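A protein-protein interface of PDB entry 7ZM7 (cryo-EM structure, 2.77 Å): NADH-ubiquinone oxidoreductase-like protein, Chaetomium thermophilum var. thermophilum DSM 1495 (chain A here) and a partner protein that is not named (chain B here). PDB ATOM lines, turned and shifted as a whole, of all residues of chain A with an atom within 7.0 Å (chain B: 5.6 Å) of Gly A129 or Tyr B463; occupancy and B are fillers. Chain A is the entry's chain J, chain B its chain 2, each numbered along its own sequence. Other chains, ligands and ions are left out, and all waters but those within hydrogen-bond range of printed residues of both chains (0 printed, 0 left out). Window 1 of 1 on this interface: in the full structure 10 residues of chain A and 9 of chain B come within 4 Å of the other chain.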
ATOM      1  N   ALA A 123      15.672 -10.835  13.436  1.00  0.00           N
ATOM      2  CA  ALA A 123      14.604 -10.638  12.468  1.00  0.00           C
ATOM      3  C   ALA A 123      13.549  -9.689  13.010  1.00  0.00           C
ATOM      4  O   ALA A 123      13.087  -8.788  12.305  1.00  0.00           O
ATOM      5  CB  ALA A 123      13.984 -11.978  12.095  1.00  0.00           C
ATOM      6  N   ALA A 126      14.894  -5.813  13.876  1.00  0.00           N
ATOM      7  CA  ALA A 126      15.090  -5.094  12.634  1.00  0.00           C
ATOM      8  C   ALA A 126      13.786  -4.767  11.941  1.00  0.00           C
ATOM      9  O   ALA A 126      13.785  -4.003  10.974  1.00  0.00           O
ATOM     10  CB  ALA A 126      15.973  -5.917  11.704  1.00  0.00           C
ATOM     11  N   GLY A 127      12.679  -5.311  12.421  1.00  0.00           N
ATOM     12  CA  GLY A 127      11.408  -5.169  11.752  1.00  0.00           C
ATOM     13  C   GLY A 127      11.095  -6.357  10.861  1.00  0.00           C
ATOM     14  O   GLY A 127      11.972  -7.100  10.423  1.00  0.00           O
ATOM     15  N   SER A 128       9.805  -6.528  10.592  1.00  0.00           N
ATOM     16  CA  SER A 128       9.347  -7.622   9.750  1.00  0.00           C
ATOM     17  C   SER A 128       9.712  -7.350   8.297  1.00  0.00           C
ATOM     18  O   SER A 128       9.010  -6.607   7.604  1.00  0.00           O
ATOM     19  CB  SER A 128       7.839  -7.815   9.904  1.00  0.00           C
ATOM     20  OG  SER A 128       7.493  -8.028  11.262  1.00  0.00           O
ATOM     21  N   GLY A 129      10.819  -7.926   7.835  1.00  0.00           N
ATOM     22  CA  GLY A 129      11.272  -7.699   6.478  1.00  0.00           C
ATOM     23  C   GLY A 129      10.621  -8.598   5.450  1.00  0.00           C
ATOM     24  O   GLY A 129      10.347  -8.165   4.331  1.00  0.00           O
ATOM     25  N   LEU A 130      10.361  -9.854   5.821  1.00  0.00           N
ATOM     26  CA  LEU A 130       9.896 -10.844   4.855  1.00  0.00           C
ATOM     27  C   LEU A 130       8.439 -10.643   4.449  1.00  0.00           C
ATOM     28  O   LEU A 130       7.999 -11.240   3.463  1.00  0.00           O
ATOM     29  CB  LEU A 130      10.119 -12.248   5.412  1.00  0.00           C
ATOM     30  CG  LEU A 130      11.603 -12.599   5.555  1.00  0.00           C
ATOM     31  CD1 LEU A 130      11.810 -14.098   5.653  1.00  0.00           C
ATOM     32  CD2 LEU A 130      12.428 -12.020   4.409  1.00  0.00           C
ATOM     33  N   ARG A 131       7.681  -9.852   5.192  1.00  0.00           N
ATOM     34  CA  ARG A 131       6.407  -9.329   4.731  1.00  0.00           C
ATOM     35  C   ARG A 131       6.571  -7.843   4.422  1.00  0.00           C
ATOM     36  O   ARG A 131       7.683  -7.335   4.266  1.00  0.00           O
ATOM     37  CB  ARG A 131       5.306  -9.564   5.765  1.00  0.00           C
ATOM     38  CG  ARG A 131       5.011 -11.016   6.075  1.00  0.00           C
ATOM     39  CD  ARG A 131       4.370 -11.718   4.896  1.00  0.00           C
ATOM     40  NE  ARG A 131       4.018 -13.098   5.216  1.00  0.00           N
ATOM     41  CZ  ARG A 131       3.506 -13.960   4.344  1.00  0.00           C
ATOM     42  NH1 ARG A 131       3.285 -13.584   3.096  1.00  0.00           N
ATOM     43  NH2 ARG A 131       3.213 -15.197   4.719  1.00  0.00           N
ATOM     44  N   GLY A 132       5.454  -7.137   4.324  1.00  0.00           N
ATOM     45  CA  GLY A 132       5.504  -5.707   4.114  1.00  0.00           C
ATOM     46  C   GLY A 132       6.163  -4.974   5.261  1.00  0.00           C
ATOM     47  O   GLY A 132       5.717  -5.074   6.408  1.00  0.00           O
ATOM     48  N   VAL A 133       7.237  -4.239   4.967  1.00  0.00           N
ATOM     49  CA  VAL A 133       7.875  -3.427   5.991  1.00  0.00           C
ATOM     50  C   VAL A 133       6.933  -2.301   6.400  1.00  0.00           C
ATOM     51  O   VAL A 133       6.168  -1.767   5.585  1.00  0.00           O
ATOM     52  CB  VAL A 133       9.230  -2.886   5.494  1.00  0.00           C
ATOM     53  CG1 VAL A 133       9.035  -1.882   4.371  1.00  0.00           C
ATOM     54  CG2 VAL A 133      10.014  -2.268   6.642  1.00  0.00           C
ATOM     55  N   LEU B 316      11.491 -11.870  -2.401  1.00  0.00           N
ATOM     56  CA  LEU B 316      12.247 -11.655  -1.137  1.00  0.00           C
ATOM     57  C   LEU B 316      12.723 -12.991  -0.562  1.00  0.00           C
ATOM     58  O   LEU B 316      13.826 -13.033  -0.014  1.00  0.00           O
ATOM     59  CB  LEU B 316      11.411 -10.875  -0.121  1.00  0.00           C
ATOM     60  CG  LEU B 316      11.673  -9.377  -0.041  1.00  0.00           C
ATOM     61  CD1 LEU B 316      10.927  -8.784   1.141  1.00  0.00           C
ATOM     62  CD2 LEU B 316      13.160  -9.093   0.077  1.00  0.00           C
ATOM     63  N   LEU B 353      16.778  -8.798  -4.492  1.00  0.00           N
ATOM     64  CA  LEU B 353      16.497  -7.911  -3.333  1.00  0.00           C
ATOM     65  C   LEU B 353      16.204  -6.481  -3.798  1.00  0.00           C
ATOM     66  O   LEU B 353      15.234  -5.902  -3.303  1.00  0.00           O
ATOM     67  CB  LEU B 353      17.665  -7.996  -2.348  1.00  0.00           C
ATOM     68  CG  LEU B 353      17.640  -7.017  -1.175  1.00  0.00           C
ATOM     69  CD1 LEU B 353      16.493  -7.327  -0.228  1.00  0.00           C
ATOM     70  CD2 LEU B 353      18.962  -7.035  -0.429  1.00  0.00           C
ATOM     71  N   SER B 356      12.744  -6.341  -5.166  1.00  0.00           N
ATOM     72  CA  SER B 356      11.718  -6.520  -4.107  1.00  0.00           C
ATOM     73  C   SER B 356      11.486  -5.239  -3.302  1.00  0.00           C
ATOM     74  O   SER B 356      10.332  -4.966  -2.959  1.00  0.00           O
ATOM     75  CB  SER B 356      12.097  -7.658  -3.213  1.00  0.00           C
ATOM     76  OG  SER B 356      12.191  -8.864  -3.944  1.00  0.00           O
ATOM     77  N   VAL B 357      12.545  -4.507  -2.981  1.00  0.00           N
ATOM     78  CA  VAL B 357      12.360  -3.210  -2.294  1.00  0.00           C
ATOM     79  C   VAL B 357      12.013  -2.277  -3.436  1.00  0.00           C
ATOM     80  O   VAL B 357      12.862  -2.101  -4.298  1.00  0.00           O
ATOM     81  CB  VAL B 357      13.693  -2.788  -1.651  1.00  0.00           C
ATOM     82  CG1 VAL B 357      13.597  -1.492  -0.867  1.00  0.00           C
ATOM     83  CG2 VAL B 357      14.334  -3.897  -0.841  1.00  0.00           C
ATOM     84  N   SER B 358      10.800  -1.759  -3.504  1.00  0.00           N
ATOM     85  CA  SER B 358      10.546  -0.893  -4.673  1.00  0.00           C
ATOM     86  C   SER B 358      10.709   0.556  -4.232  1.00  0.00           C
ATOM     87  O   SER B 358       9.752   1.103  -3.667  1.00  0.00           O
ATOM     88  CB  SER B 358       9.214  -1.168  -5.280  1.00  0.00           C
ATOM     89  OG  SER B 358       9.177  -0.742  -6.633  1.00  0.00           O
ATOM     90  N   ALA B 457      20.237   0.883  -0.684  1.00  0.00           N
ATOM     91  CA  ALA B 457      18.798   0.920  -0.983  1.00  0.00           C
ATOM     92  C   ALA B 457      18.031   0.124   0.069  1.00  0.00           C
ATOM     93  O   ALA B 457      16.997   0.615   0.533  1.00  0.00           O
ATOM     94  CB  ALA B 457      18.654   0.288  -2.321  1.00  0.00           C
ATOM     95  N   ALA B 458      18.516  -1.072   0.410  1.00  0.00           N
ATOM     96  CA  ALA B 458      17.837  -1.948   1.385  1.00  0.00           C
ATOM     97  C   ALA B 458      17.866  -1.346   2.785  1.00  0.00           C
ATOM     98  O   ALA B 458      16.827  -1.341   3.436  1.00  0.00           O
ATOM     99  CB  ALA B 458      18.522  -3.269   1.360  1.00  0.00           C
ATOM    100  N   LEU B 459      19.000  -0.791   3.186  1.00  0.00           N
ATOM    101  CA  LEU B 459      19.153  -0.221   4.538  1.00  0.00           C
ATOM    102  C   LEU B 459      18.298   1.030   4.684  1.00  0.00           C
ATOM    103  O   LEU B 459      17.750   1.243   5.768  1.00  0.00           O
ATOM    104  CB  LEU B 459      20.628   0.153   4.687  1.00  0.00           C
ATOM    105  CG  LEU B 459      21.585  -0.977   5.041  1.00  0.00           C
ATOM    106  CD1 LEU B 459      23.019  -0.492   4.918  1.00  0.00           C
ATOM    107  CD2 LEU B 459      21.310  -1.497   6.443  1.00  0.00           C
ATOM    108  N   ASN B 461      15.548   1.686   3.338  1.00  0.00           N
ATOM    109  CA  ASN B 461      14.094   1.381   3.346  1.00  0.00           C
ATOM    110  C   ASN B 461      13.732   0.271   4.338  1.00  0.00           C
ATOM    111  O   ASN B 461      12.608  -0.247   4.240  1.00  0.00           O
ATOM    112  CB  ASN B 461      13.590   1.004   1.953  1.00  0.00           C
ATOM    113  CG  ASN B 461      12.225   1.572   1.632  1.00  0.00           C
ATOM    114  OD1 ASN B 461      11.804   2.562   2.226  1.00  0.00           O
ATOM    115  ND2 ASN B 461      11.531   0.957   0.690  1.00  0.00           N
ATOM    116  N   GLY B 462      14.636  -0.113   5.236  1.00  0.00           N
ATOM    117  CA  GLY B 462      14.206  -1.082   6.269  1.00  0.00           C
ATOM    118  C   GLY B 462      14.511  -2.553   6.044  1.00  0.00           C
ATOM    119  O   GLY B 462      13.868  -3.367   6.705  1.00  0.00           O
ATOM    120  N   TYR B 463      15.504  -2.887   5.240  1.00  0.00           N
ATOM    121  CA  TYR B 463      15.795  -4.302   4.902  1.00  0.00           C
ATOM    122  C   TYR B 463      17.104  -4.677   5.590  1.00  0.00           C
ATOM    123  O   TYR B 463      17.826  -5.531   5.082  1.00  0.00           O
ATOM    124  CB  TYR B 463      15.619  -4.595   3.414  1.00  0.00           C
ATOM    125  CG  TYR B 463      14.219  -4.469   2.877  1.00  0.00           C
ATOM    126  CD1 TYR B 463      13.669  -3.231   2.589  1.00  0.00           C
ATOM    127  CD2 TYR B 463      13.451  -5.592   2.629  1.00  0.00           C
ATOM    128  CE1 TYR B 463      12.383  -3.109   2.089  1.00  0.00           C
ATOM    129  CE2 TYR B 463      12.169  -5.489   2.124  1.00  0.00           C
ATOM    130  CZ  TYR B 463      11.634  -4.245   1.851  1.00  0.00           C
ATOM    131  OH  TYR B 463      10.370  -4.148   1.354  1.00  0.00           O
ATOM    132  N   ILE B 464      17.401  -3.992   6.685  1.00  0.00           N
ATOM    133  CA  ILE B 464      18.568  -4.306   7.550  1.00  0.00           C
ATOM    134  C   ILE B 464      18.764  -5.813   7.735  1.00  0.00           C
ATOM    135  O   ILE B 464      19.927  -6.244   7.696  1.00  0.00           O
ATOM    136  CB  ILE B 464      18.369  -3.572   8.896  1.00  0.00           C
ATOM    137  CG1 ILE B 464      19.306  -4.076   9.995  1.00  0.00           C
ATOM    138  CG2 ILE B 464      16.914  -3.580   9.321  1.00  0.00           C
ATOM    139  CD1 ILE B 464      20.640  -3.370  10.026  1.00  0.00           C
ATOM    140  N   PHE B 465      17.708  -6.602   7.947  1.00  0.00           N
ATOM    141  CA  PHE B 465      17.941  -8.046   8.229  1.00  0.00           C
ATOM    142  C   PHE B 465      18.568  -8.717   7.006  1.00  0.00           C
ATOM    143  O   PHE B 465      19.554  -9.448   7.173  1.00  0.00           O
ATOM    144  CB  PHE B 465      16.670  -8.751   8.707  1.00  0.00           C
ATOM    145  CG  PHE B 465      16.796 -10.250   8.823  1.00  0.00           C
ATOM    146  CD1 PHE B 465      17.489 -10.822   9.876  1.00  0.00           C
ATOM    147  CD2 PHE B 465      16.227 -11.086   7.877  1.00  0.00           C
ATOM    148  CE1 PHE B 465      17.609 -12.199   9.981  1.00  0.00           C
ATOM    149  CE2 PHE B 465      16.348 -12.462   7.983  1.00  0.00           C
ATOM    150  CZ  PHE B 465      17.038 -13.015   9.035  1.00  0.00           C
ATOM    151  N   LEU B 466      18.013  -8.468   5.821  1.00  0.00           N
ATOM    152  CA  LEU B 466      18.544  -9.058   4.564  1.00  0.00           C
ATOM    153  C   LEU B 466      19.956  -8.546   4.252  1.00  0.00           C
ATOM    154  O   LEU B 466      20.760  -9.355   3.781  1.00  0.00           O
ATOM    155  CB  LEU B 466      17.557  -8.788   3.428  1.00  0.00           C
ATOM    156  CG  LEU B 466      16.328  -9.694   3.422  1.00  0.00           C
ATOM    157  CD1 LEU B 466      15.049  -8.879   3.332  1.00  0.00           C
ATOM    158  CD2 LEU B 466      16.403 -10.708   2.292  1.00  0.00           C
ATOM    159  N   SER B 467      20.235  -7.263   4.485  1.00  0.00           N
ATOM    160  CA  SER B 467      21.594  -6.697   4.260  1.00  0.00           C
ATOM    161  C   SER B 467      22.650  -7.490   5.044  1.00  0.00           C
ATOM    162  O   SER B 467      23.671  -7.842   4.443  1.00  0.00           O
ATOM    163  CB  SER B 467      21.630  -5.235   4.620  1.00  0.00           C
ATOM    164  OG  SER B 467      20.633  -4.514   3.912  1.00  0.00           O
ATOM    165  N   LEU B 468      22.421  -7.735   6.337  1.00  0.00           N
ATOM    166  CA  LEU B 468      23.355  -8.509   7.192  1.00  0.00           C
ATOM    167  C   LEU B 468      23.503  -9.928   6.648  1.00  0.00           C
ATOM    168  O   LEU B 468      24.610 -10.472   6.762  1.00  0.00           O
ATOM    169  CB  LEU B 468      22.787  -8.549   8.608  1.00  0.00           C
ATOM    170  CG  LEU B 468      22.833  -7.236   9.385  1.00  0.00           C
ATOM    171  CD1 LEU B 468      21.870  -7.275  10.560  1.00  0.00           C
ATOM    172  CD2 LEU B 468      24.244  -6.944   9.866  1.00  0.00           C
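Of the 16 printed residues of chain B, 5 touch a printed residue of chain A. Of the 9 printed residues of chain A, 4 touch a printed residue of chain B. Printed residues of chain A that touch a printed residue of chain B: Ala A123, Ala A126, Gly A129 and Val A133.
Among the printed residues, pairs that only touch across the chains: Gly A129 with Leu B316, Ala A126 with Ile B464, Ala A123 with Phe B465, Gly A129 with Tyr B463 and Val A133 with Asn B461.
The backbone carbonyl oxygen of Ala B458 sits at hydrogen-bond distance from the backbone NH of Tyr B463, at 2.7 Å. The side-chain hydroxyl (OG) of Ser B356 sits at hydrogen-bond distance from the backbone NH (N) of Leu B316 (3.5 Å). The side-chain hydroxyl (OG) of Ser B467 sits at hydrogen-bond distance from the backbone carbonyl oxygen (O) of Tyr B463 (3.2 Å).
Of the printed residues of chain B, Ala A123 touches Phe B465. Of the printed residues of chain B, Ala A126 touches Ile B464. Of chain B, only Leu B316 (3.3 Å) and Tyr B463 (3.9 Å) come within 4 Å of Gly A129. Printed residues of chain A within 4 Å of Leu B316: Gly A129. Ser B356 touches none of the printed residues of chain A. Val B357 touches none of the printed residues of chain A. Of the printed residues of chain A, Asn B461 touches Val A133. Printed residues of chain A within 4 Å of Tyr B463: Gly A129 (3.9 Å). The nearest residue of chain B that does not touch Gly A129 is Leu B466 (4.9 Å). The nearest printed residue of chain A that does not touch Tyr B463 is Val A133 (4.002 Å).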
